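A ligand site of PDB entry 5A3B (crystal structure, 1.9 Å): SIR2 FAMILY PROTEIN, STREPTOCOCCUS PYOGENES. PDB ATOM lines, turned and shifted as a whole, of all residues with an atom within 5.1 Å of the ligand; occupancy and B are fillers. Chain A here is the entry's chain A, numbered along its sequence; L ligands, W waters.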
ATOM      1  N   GLY A  43      11.336  -3.626 -15.645  1.00  0.00           N
ATOM      2  CA  GLY A  43      11.363  -4.880 -14.982  1.00  0.00           C
ATOM      3  C   GLY A  43      11.069  -6.053 -15.890  1.00  0.00           C
ATOM      4  O   GLY A  43      11.036  -5.949 -17.116  1.00  0.00           O
ATOM      5  N   ALA A  44      10.839  -7.188 -15.240  1.00  0.00           N
ATOM      6  CA  ALA A  44      10.840  -8.483 -15.950  1.00  0.00           C
ATOM      7  C   ALA A  44       9.699  -8.597 -16.937  1.00  0.00           C
ATOM      8  O   ALA A  44       9.789  -9.361 -17.904  1.00  0.00           O
ATOM      9  CB  ALA A  44      10.812  -9.617 -14.959  1.00  0.00           C
ATOM     10  N   GLY A  45       8.634  -7.850 -16.736  1.00  0.00           N
ATOM     11  CA  GLY A  45       7.503  -7.833 -17.678  1.00  0.00           C
ATOM     12  C   GLY A  45       7.863  -7.454 -19.101  1.00  0.00           C
ATOM     13  O   GLY A  45       7.286  -7.984 -20.035  1.00  0.00           O
ATOM     14  N   ALA A  48       9.455 -10.598 -20.521  1.00  0.00           N
ATOM     15  CA  ALA A  48       8.390 -11.580 -20.693  1.00  0.00           C
ATOM     16  C   ALA A  48       7.545 -11.259 -21.909  1.00  0.00           C
ATOM     17  O   ALA A  48       7.146 -12.148 -22.676  1.00  0.00           O
ATOM     18  CB  ALA A  48       7.511 -11.632 -19.442  1.00  0.00           C
ATOM     19  N   ALA A  49       7.259  -9.979 -22.104  1.00  0.00           N
ATOM     20  CA  ALA A  49       6.414  -9.547 -23.240  1.00  0.00           C
ATOM     21  C   ALA A  49       7.017  -9.864 -24.605  1.00  0.00           C
ATOM     22  O   ALA A  49       6.282 -10.051 -25.588  1.00  0.00           O
ATOM     23  CB  ALA A  49       6.104  -8.068 -23.123  1.00  0.00           C
ATOM     24  N   LEU A  76      12.944 -18.507 -12.197  1.00  0.00           N
ATOM     25  CA  LEU A  76      13.365 -17.607 -11.143  1.00  0.00           C
ATOM     26  C   LEU A  76      13.646 -18.329  -9.819  1.00  0.00           C
ATOM     27  O   LEU A  76      14.699 -18.192  -9.194  1.00  0.00           O
ATOM     28  CB  LEU A  76      12.283 -16.555 -10.900  1.00  0.00           C
ATOM     29  CG  LEU A  76      12.638 -15.489  -9.867  1.00  0.00           C
ATOM     30  CD1 LEU A  76      13.864 -14.731 -10.364  1.00  0.00           C
ATOM     31  CD2 LEU A  76      11.443 -14.559  -9.611  1.00  0.00           C
ATOM     32  N   THR A 127      15.878  -3.558 -13.156  1.00  0.00           N
ATOM     33  CA  THR A 127      16.157  -4.698 -12.289  1.00  0.00           C
ATOM     34  C   THR A 127      16.423  -5.989 -13.055  1.00  0.00           C
ATOM     35  O   THR A 127      16.792  -7.016 -12.458  1.00  0.00           O
ATOM     36  CB  THR A 127      15.018  -4.901 -11.264  1.00  0.00           C
ATOM     37  OG1 THR A 127      13.751  -4.993 -11.935  1.00  0.00           O
ATOM     38  CG2 THR A 127      14.969  -3.732 -10.310  1.00  0.00           C
ATOM     39  N   ASN A 128      16.285  -5.945 -14.387  1.00  0.00           N
ATOM     40  CA  ASN A 128      16.571  -7.093 -15.225  1.00  0.00           C
ATOM     41  C   ASN A 128      18.067  -7.335 -15.315  1.00  0.00           C
ATOM     42  O   ASN A 128      18.848  -6.394 -15.263  1.00  0.00           O
ATOM     43  CB  ASN A 128      16.039  -6.863 -16.631  1.00  0.00           C
ATOM     44  CG  ASN A 128      14.519  -6.884 -16.705  1.00  0.00           C
ATOM     45  OD1 ASN A 128      13.848  -7.270 -15.745  1.00  0.00           O
ATOM     46  ND2 ASN A 128      13.981  -6.518 -17.840  1.00  0.00           N
ATOM     47  N   GLN A 147      20.534  -4.526 -10.320  1.00  0.00           N
ATOM     48  CA  GLN A 147      20.535  -5.916  -9.819  1.00  0.00           C
ATOM     49  C   GLN A 147      21.611  -6.781 -10.437  1.00  0.00           C
ATOM     50  O   GLN A 147      21.491  -8.030 -10.441  1.00  0.00           O
ATOM     51  CB  GLN A 147      19.150  -6.571 -10.133  1.00  0.00           C
ATOM     52  CG  GLN A 147      18.031  -6.032  -9.307  1.00  0.00           C
ATOM     53  CD  GLN A 147      18.125  -6.502  -7.879  1.00  0.00           C
ATOM     54  OE1 GLN A 147      19.001  -6.052  -7.123  1.00  0.00           O
ATOM     55  NE2 GLN A 147      17.232  -7.438  -7.472  1.00  0.00           N
ATOM     56  N   TYR A 150      23.661 -11.169 -15.494  1.00  0.00           N
ATOM     57  CA  TYR A 150      23.934 -12.604 -15.453  1.00  0.00           C
ATOM     58  C   TYR A 150      25.284 -12.988 -16.054  1.00  0.00           C
ATOM     59  O   TYR A 150      25.831 -14.037 -15.710  1.00  0.00           O
ATOM     60  CB  TYR A 150      22.842 -13.422 -16.179  1.00  0.00           C
ATOM     61  CG  TYR A 150      21.467 -13.296 -15.622  1.00  0.00           C
ATOM     62  CD1 TYR A 150      21.221 -13.286 -14.236  1.00  0.00           C
ATOM     63  CD2 TYR A 150      20.365 -13.196 -16.490  1.00  0.00           C
ATOM     64  CE1 TYR A 150      19.922 -13.195 -13.746  1.00  0.00           C
ATOM     65  CE2 TYR A 150      19.076 -13.071 -16.008  1.00  0.00           C
ATOM     66  CZ  TYR A 150      18.860 -13.091 -14.657  1.00  0.00           C
ATOM     67  OH  TYR A 150      17.568 -12.987 -14.224  1.00  0.00           O
ATOM     68  N   GLY A 239       6.531  -3.051 -16.797  1.00  0.00           N
ATOM     69  CA  GLY A 239       6.583  -4.465 -16.444  1.00  0.00           C
ATOM     70  C   GLY A 239       7.297  -4.709 -15.134  1.00  0.00           C
ATOM     71  O   GLY A 239       8.045  -5.664 -15.003  1.00  0.00           O
ATOM     72  N   VAL A 240       7.026  -3.837 -14.181  1.00  0.00           N
ATOM     73  CA  VAL A 240       7.559  -3.924 -12.844  1.00  0.00           C
ATOM     74  C   VAL A 240       6.469  -4.392 -11.908  1.00  0.00           C
ATOM     75  O   VAL A 240       5.417  -3.787 -11.847  1.00  0.00           O
ATOM     76  CB  VAL A 240       8.082  -2.552 -12.380  1.00  0.00           C
ATOM     77  CG1 VAL A 240       8.363  -2.527 -10.895  1.00  0.00           C
ATOM     78  CG2 VAL A 240       9.329  -2.182 -13.206  1.00  0.00           C
ATOM     79  N   GLY A 241       6.775  -5.425 -11.138  1.00  0.00           N
ATOM     80  CA  GLY A 241       5.795  -6.049 -10.262  1.00  0.00           C
ATOM     81  C   GLY A 241       6.095  -5.817  -8.780  1.00  0.00           C
ATOM     82  O   GLY A 241       6.677  -4.799  -8.385  1.00  0.00           O
ATOM     83  N   HIS A 242       5.680  -6.787  -7.966  1.00  0.00           N
ATOM     84  CA  HIS A 242       5.820  -6.708  -6.515  1.00  0.00           C
ATOM     85  C   HIS A 242       7.030  -7.430  -5.968  1.00  0.00           C
ATOM     86  O   HIS A 242       7.249  -7.394  -4.764  1.00  0.00           O
ATOM     87  CB  HIS A 242       4.593  -7.317  -5.834  1.00  0.00           C
ATOM     88  CG  HIS A 242       3.720  -6.308  -5.152  1.00  0.00           C
ATOM     89  ND1 HIS A 242       2.685  -6.684  -4.322  1.00  0.00           N
ATOM     90  CD2 HIS A 242       3.716  -4.958  -5.174  1.00  0.00           C
ATOM     91  CE1 HIS A 242       2.069  -5.601  -3.861  1.00  0.00           C
ATOM     92  NE2 HIS A 242       2.684  -4.543  -4.365  1.00  0.00           N
ATOM     93  N   THR A 243       7.816  -8.098  -6.802  1.00  0.00           N
ATOM     94  CA  THR A 243       8.886  -8.953  -6.299  1.00  0.00           C
ATOM     95  C   THR A 243       9.949  -8.155  -5.506  1.00  0.00           C
ATOM     96  O   THR A 243      10.359  -8.610  -4.443  1.00  0.00           O
ATOM     97  CB  THR A 243       9.559  -9.721  -7.455  1.00  0.00           C
ATOM     98  OG1 THR A 243       8.545 -10.391  -8.225  1.00  0.00           O
ATOM     99  CG2 THR A 243      10.581 -10.740  -6.946  1.00  0.00           C
ATOM    100  N   THR A 244      10.367  -7.003  -6.017  1.00  0.00           N
ATOM    101  CA  THR A 244      11.380  -6.137  -5.361  1.00  0.00           C
ATOM    102  C   THR A 244      11.070  -4.652  -5.605  1.00  0.00           C
ATOM    103  O   THR A 244      11.850  -3.926  -6.279  1.00  0.00           O
ATOM    104  CB  THR A 244      12.827  -6.412  -5.865  1.00  0.00           C
ATOM    105  OG1 THR A 244      12.892  -6.264  -7.297  1.00  0.00           O
ATOM    106  CG2 THR A 244      13.305  -7.826  -5.464  1.00  0.00           C
ATOM    107  N   PHE A 247      13.393  -1.069  -5.601  1.00  0.00           N
ATOM    108  CA  PHE A 247      14.372  -0.543  -6.561  1.00  0.00           C
ATOM    109  C   PHE A 247      13.799   0.437  -7.553  1.00  0.00           C
ATOM    110  O   PHE A 247      14.433   1.458  -7.855  1.00  0.00           O
ATOM    111  CB  PHE A 247      15.085  -1.691  -7.277  1.00  0.00           C
ATOM    112  CG  PHE A 247      15.846  -2.569  -6.338  1.00  0.00           C
ATOM    113  CD1 PHE A 247      16.905  -2.037  -5.595  1.00  0.00           C
ATOM    114  CD2 PHE A 247      15.482  -3.887  -6.137  1.00  0.00           C
ATOM    115  CE1 PHE A 247      17.610  -2.812  -4.695  1.00  0.00           C
ATOM    116  CE2 PHE A 247      16.197  -4.664  -5.246  1.00  0.00           C
ATOM    117  CZ  PHE A 247      17.237  -4.129  -4.514  1.00  0.00           C
ATOM    118  N   LEU A 267       3.071   0.687 -17.262  1.00  0.00           N
ATOM    119  CA  LEU A 267       2.679  -0.276 -18.263  1.00  0.00           C
ATOM    120  C   LEU A 267       2.679  -1.612 -17.570  1.00  0.00           C
ATOM    121  O   LEU A 267       3.757  -2.213 -17.317  1.00  0.00           O
ATOM    122  CB  LEU A 267       3.670  -0.307 -19.421  1.00  0.00           C
ATOM    123  CG  LEU A 267       3.447   0.690 -20.518  1.00  0.00           C
ATOM    124  CD1 LEU A 267       3.287   2.096 -19.995  1.00  0.00           C
ATOM    125  CD2 LEU A 267       4.545   0.632 -21.540  1.00  0.00           C
ATOM    126  N   ASN A 268       1.487  -2.117 -17.306  1.00  0.00           N
ATOM    127  CA  ASN A 268       1.372  -3.350 -16.589  1.00  0.00           C
ATOM    128  C   ASN A 268      -0.006  -3.929 -16.819  1.00  0.00           C
ATOM    129  O   ASN A 268      -1.011  -3.242 -16.614  1.00  0.00           O
ATOM    130  CB  ASN A 268       1.609  -3.128 -15.099  1.00  0.00           C
ATOM    131  CG  ASN A 268       2.053  -4.394 -14.405  1.00  0.00           C
ATOM    132  OD1 ASN A 268       1.373  -5.415 -14.428  1.00  0.00           O
ATOM    133  ND2 ASN A 268       3.216  -4.351 -13.801  1.00  0.00           N
ATOM    134  N   HIS A 269      -0.065  -5.207 -17.175  1.00  0.00           N
ATOM    135  CA  HIS A 269      -1.368  -5.866 -17.320  1.00  0.00           C
ATOM    136  C   HIS A 269      -2.058  -6.257 -16.009  1.00  0.00           C
ATOM    137  O   HIS A 269      -3.199  -6.653 -16.075  1.00  0.00           O
ATOM    138  CB  HIS A 269      -1.401  -6.982 -18.402  1.00  0.00           C
ATOM    139  CG  HIS A 269      -0.531  -8.193 -18.142  1.00  0.00           C
ATOM    140  ND1 HIS A 269      -0.296  -9.125 -19.139  1.00  0.00           N
ATOM    141  CD2 HIS A 269       0.114  -8.650 -17.041  1.00  0.00           C
ATOM    142  CE1 HIS A 269       0.467 -10.098 -18.660  1.00  0.00           C
ATOM    143  NE2 HIS A 269       0.734  -9.834 -17.394  1.00  0.00           N
ATOM    144  N   LYS A 270      -1.391  -6.119 -14.848  1.00  0.00           N
ATOM    145  CA  LYS A 270      -2.032  -6.274 -13.526  1.00  0.00           C
ATOM    146  C   LYS A 270      -2.149  -4.926 -12.803  1.00  0.00           C
ATOM    147  O   LYS A 270      -1.367  -4.003 -13.075  1.00  0.00           O
ATOM    148  CB  LYS A 270      -1.246  -7.274 -12.659  1.00  0.00           C
ATOM    149  CG  LYS A 270      -1.321  -8.679 -13.220  1.00  0.00           C
ATOM    150  CD  LYS A 270      -0.584  -9.708 -12.366  1.00  0.00           C
ATOM    151  CE  LYS A 270      -1.104 -11.118 -12.654  1.00  0.00           C
ATOM    152  NZ  LYS A 270      -1.544 -11.814 -11.391  1.00  0.00           N
ATOM    153  N   TYR A 272      -1.603  -2.635  -9.625  1.00  0.00           N
ATOM    154  CA  TYR A 272      -0.954  -2.446  -8.330  1.00  0.00           C
ATOM    155  C   TYR A 272      -1.417  -1.077  -7.834  1.00  0.00           C
ATOM    156  O   TYR A 272      -1.295  -0.085  -8.544  1.00  0.00           O
ATOM    157  CB  TYR A 272       0.567  -2.514  -8.462  1.00  0.00           C
ATOM    158  CG  TYR A 272       1.047  -3.847  -8.989  1.00  0.00           C
ATOM    159  CD1 TYR A 272       0.981  -4.138 -10.350  1.00  0.00           C
ATOM    160  CD2 TYR A 272       1.549  -4.812  -8.135  1.00  0.00           C
ATOM    161  CE1 TYR A 272       1.414  -5.366 -10.835  1.00  0.00           C
ATOM    162  CE2 TYR A 272       1.981  -6.040  -8.620  1.00  0.00           C
ATOM    163  CZ  TYR A 272       1.917  -6.297  -9.966  1.00  0.00           C
ATOM    164  OH  TYR A 272       2.358  -7.512 -10.435  1.00  0.00           O
ATOM    165  N   THR A 286      -2.841  -0.953 -19.435  1.00  0.00           N
ATOM    166  CA  THR A 286      -2.909  -2.383 -19.265  1.00  0.00           C
ATOM    167  C   THR A 286      -2.671  -3.200 -20.530  1.00  0.00           C
ATOM    168  O   THR A 286      -2.551  -4.408 -20.427  1.00  0.00           O
ATOM    169  CB  THR A 286      -4.252  -2.817 -18.688  1.00  0.00           C
ATOM    170  OG1 THR A 286      -5.278  -2.223 -19.471  1.00  0.00           O
ATOM    171  CG2 THR A 286      -4.368  -2.415 -17.252  1.00  0.00           C
ATOM    172  N   GLU A 287      -2.571  -2.562 -21.700  1.00  0.00           N
ATOM    173  CA  GLU A 287      -2.374  -3.296 -22.953  1.00  0.00           C
ATOM    174  C   GLU A 287      -1.049  -4.077 -22.952  1.00  0.00           C
ATOM    175  O   GLU A 287      -0.045  -3.592 -22.462  1.00  0.00           O
ATOM    176  CB  GLU A 287      -2.389  -2.324 -24.138  1.00  0.00           C
ATOM    177  CG  GLU A 287      -2.270  -2.998 -25.495  1.00  0.00           C
ATOM    178  CD  GLU A 287      -2.433  -2.038 -26.656  1.00  0.00           C
ATOM    179  OE1 GLU A 287      -2.930  -0.893 -26.446  1.00  0.00           O
ATOM    180  OE2 GLU A 287      -2.075  -2.447 -27.791  1.00  0.00           O
ATOM    181  N   HIS A 288      -1.040  -5.270 -23.542  1.00  0.00           N
ATOM    182  CA  HIS A 288       0.173  -6.078 -23.579  1.00  0.00           C
ATOM    183  C   HIS A 288       1.353  -5.204 -23.995  1.00  0.00           C
ATOM    184  O   HIS A 288       1.304  -4.525 -25.010  1.00  0.00           O
ATOM    185  CB  HIS A 288      -0.071  -7.238 -24.559  1.00  0.00           C
ATOM    186  CG  HIS A 288       1.039  -8.243 -24.640  1.00  0.00           C
ATOM    187  ND1 HIS A 288       2.265  -7.961 -25.203  1.00  0.00           N
ATOM    188  CD2 HIS A 288       1.065  -9.559 -24.325  1.00  0.00           C
ATOM    189  CE1 HIS A 288       3.022  -9.054 -25.196  1.00  0.00           C
ATOM    190  NE2 HIS A 288       2.318 -10.035 -24.658  1.00  0.00           N
ATOM    191  N   ILE A 289       2.391  -5.166 -23.170  1.00  0.00           N
ATOM    192  CA  ILE A 289       3.551  -4.300 -23.399  1.00  0.00           C
ATOM    193  C   ILE A 289       4.091  -4.322 -24.850  1.00  0.00           C
ATOM    194  O   ILE A 289       4.352  -3.267 -25.430  1.00  0.00           O
ATOM    195  CB  ILE A 289       4.689  -4.644 -22.391  1.00  0.00           C
ATOM    196  CG1 ILE A 289       4.346  -4.070 -21.018  1.00  0.00           C
ATOM    197  CG2 ILE A 289       6.055  -4.132 -22.856  1.00  0.00           C
ATOM    198  CD1 ILE A 289       5.159  -4.676 -19.888  1.00  0.00           C
HETATM  199  N1  LIG L   1       2.248  -6.741 -20.573  1.00  0.00           N
HETATM  200  C1  LIG L   1       2.151  -5.955 -19.474  1.00  0.00           C
HETATM  201  N2  LIG L   1       2.603  -6.344 -18.269  1.00  0.00           N
HETATM  202  C2  LIG L   1       3.222  -7.533 -18.098  1.00  0.00           C
HETATM  203  C3  LIG L   1       3.353  -8.442 -19.249  1.00  0.00           C
HETATM  204  C4  LIG L   1       2.825  -7.957 -20.512  1.00  0.00           C
HETATM  205  N3  LIG L   1       2.923  -8.746 -21.567  1.00  0.00           N
HETATM  206  N4  LIG L   1       3.994  -9.548 -18.817  1.00  0.00           N
HETATM  207  C5  LIG L   1       4.249  -9.365 -17.495  1.00  0.00           C
HETATM  208  N5  LIG L   1       3.774  -8.177 -17.086  1.00  0.00           N
HETATM  209  C6  LIG L   1       3.878  -7.621 -15.711  1.00  0.00           C
HETATM  210  C7  LIG L   1       3.331  -8.510 -14.609  1.00  0.00           C
HETATM  211  O1  LIG L   1       1.934  -8.333 -14.331  1.00  0.00           O
HETATM  212  C8  LIG L   1       4.183  -8.119 -13.404  1.00  0.00           C
HETATM  213  O2  LIG L   1       3.575  -7.081 -12.638  1.00  0.00           O
HETATM  214  O3  LIG L   1       5.262  -7.455 -15.428  1.00  0.00           O
HETATM  215  C9  LIG L   1       5.490  -7.598 -14.004  1.00  0.00           C
HETATM  216  C10 LIG L   1       6.619  -8.527 -13.670  1.00  0.00           C
HETATM  217  O4  LIG L   1       6.743  -8.464 -12.243  1.00  0.00           O
HETATM  218  P1  LIG L   1       7.824  -9.329 -11.418  1.00  0.00           P
HETATM  219  O5  LIG L   1       7.803 -10.713 -11.999  1.00  0.00           O
HETATM  220  O6  LIG L   1       7.695  -8.921  -9.985  1.00  0.00           O
HETATM  221  O7  LIG L   1       9.192  -8.748 -12.000  1.00  0.00           O
HETATM  222  P2  LIG L   1      10.088  -7.535 -11.466  1.00  0.00           P
HETATM  223  O8  LIG L   1       9.307  -6.342 -10.963  1.00  0.00           O
HETATM  224  O9  LIG L   1      11.093  -7.291 -12.545  1.00  0.00           O
HETATM  225  O10 LIG L   1      10.837  -8.196 -10.206  1.00  0.00           O
HETATM  226  C11 LIG L   1      11.764  -9.262 -10.401  1.00  0.00           C
HETATM  227  O11 LIG L   1      13.361 -10.510  -9.189  1.00  0.00           O
HETATM  228  O12 LIG L   1      14.702 -11.688 -10.761  1.00  0.00           O
HETATM  229  C12 LIG L   1      14.653 -10.603  -9.819  1.00  0.00           C
HETATM  230  O13 LIG L   1      16.261  -8.883 -10.630  1.00  0.00           O
HETATM  231  C13 LIG L   1      14.874  -9.273 -10.561  1.00  0.00           C
HETATM  232  O14 LIG L   1      14.698  -7.755  -8.661  1.00  0.00           O
HETATM  233  C14 LIG L   1      14.000  -8.312  -9.786  1.00  0.00           C
HETATM  234  C15 LIG L   1      12.849  -9.189  -9.340  1.00  0.00           C
HETATM  235  O   HOH W   1       4.188 -11.246 -21.090  1.00  0.00           O
HETATM  236  O   HOH W   2       9.649  -5.626  -8.135  1.00  0.00           O
HETATM  237  O   HOH W   3       1.012  -2.730 -20.180  1.00  0.00           O
HETATM  238  O   HOH W   4      11.586  -4.461 -10.327  1.00  0.00           O
HETATM  239  O   HOH W   5      13.612  -7.454 -13.106  1.00  0.00           O
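Water W5 lies within hydrogen-bond range of an oxygen (O9) of the ligand (2.6 Å), the side-chain amide oxygen of Asn 128 (2.7 Å) and the side-chain hydroxyl of Thr 127 (2.7 Å).
Water W1 lies within hydrogen-bond range of a nitrogen (N3) of the ligand (2.8 Å), the backbone NH (N) of Ala 49 (3.5 Å) and the backbone carbonyl oxygen (O) of Ala 48 (3.5 Å).
Water W2 lies within hydrogen-bond range of N of Thr 244, O8 of the ligand, O of Gly 241 and N of Thr 243.
Water W4 bridges OG1 of Thr 127 (2.7 Å) and O8 of the ligand (3.0 Å).
Water W3 bridges the backbone carbonyl oxygen (O) of Glu 287 (2.7 Å) and the backbone NH (N) of Asn 268 (3.0 Å).
O of Gly 239 sits at hydrogen-bond distance from N of Ala 44 (3.2 Å).
N of Ala 44 is in hydrogen-bond range of OD1 of Asn 128 (3.1 Å).
OD1 of Asn 268 is in hydrogen-bond range of N of Lys 270 (2.9 Å).
The backbone carbonyl oxygen (O) of Val 240 lies within hydrogen-bond range of the side-chain amide nitrogen (ND2) of Asn 268 (3.0 Å).
The backbone NH of Gly 45 sits at hydrogen-bond distance from the backbone carbonyl oxygen of Gly 239 (2.9 Å).
The backbone NH (N) of Gly 239 sits at hydrogen-bond distance from the backbone carbonyl oxygen (O) of Leu 267, 2.9 Å away.
O of Gly 43 is in hydrogen-bond range of ND2 of Asn 128 (3.1 Å).
The backbone NH of Thr 243 lies close to an oxygen (O6) of the ligand (3.3 Å).
O6 of the ligand sits at hydrogen-bond distance from OG1 of Thr 243 (2.4 Å).
O2 of the ligand sits at hydrogen-bond distance from OH of Tyr 272.
The backbone carbonyl oxygen (O) of Thr 127 lies within hydrogen-bond range of an oxygen (O13) of the ligand.
The backbone NH (N) of Gly 241 lies within hydrogen-bond range of an oxygen (O8) of the ligand (2.7 Å).
An oxygen (O9) of the ligand is in hydrogen-bond range of the backbone NH (N) of Ala 44.
OG1 of Thr 244 is in hydrogen-bond range of O14 of the ligand (2.7 Å).
The side-chain amide nitrogen (NE2) of Gln 147 sits at hydrogen-bond distance from an oxygen (O14) of the ligand, 2.8 Å away.
An oxygen (O1) of the ligand is in hydrogen-bond range of the side-chain amide oxygen (OD1) of Asn 268 (3.0 Å).
N1 of the ligand is in hydrogen-bond range of N of Ile 289 (3.0 Å).
The backbone NH (N) of His 269 sits at hydrogen-bond distance from a nitrogen (N2) of the ligand (3.1 Å).
A nitrogen (N3) of the ligand lies within hydrogen-bond range of a ring nitrogen (NE2) of His 288, 3.4 Å away.
An oxygen (O3) of the ligand lies close to the backbone carbonyl oxygen of Gly 239 (3.3 Å).
Merely in contact with the ligand: Gly 43, Gly 45, Ala 49, Leu 76, Val 240, His 242 and Lys 270.
Hydrophobic or aromatic side chains that line the ligand: Ala 44, Ala 49, Leu 76, Val 240, His 269, Tyr 272, His 288 and Ile 289.
Of the 26 residues printed, 19 come within 4 Å of the ligand.
The nearest printed residue that does not touch the ligand is Ala 48 (4.1 Å).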
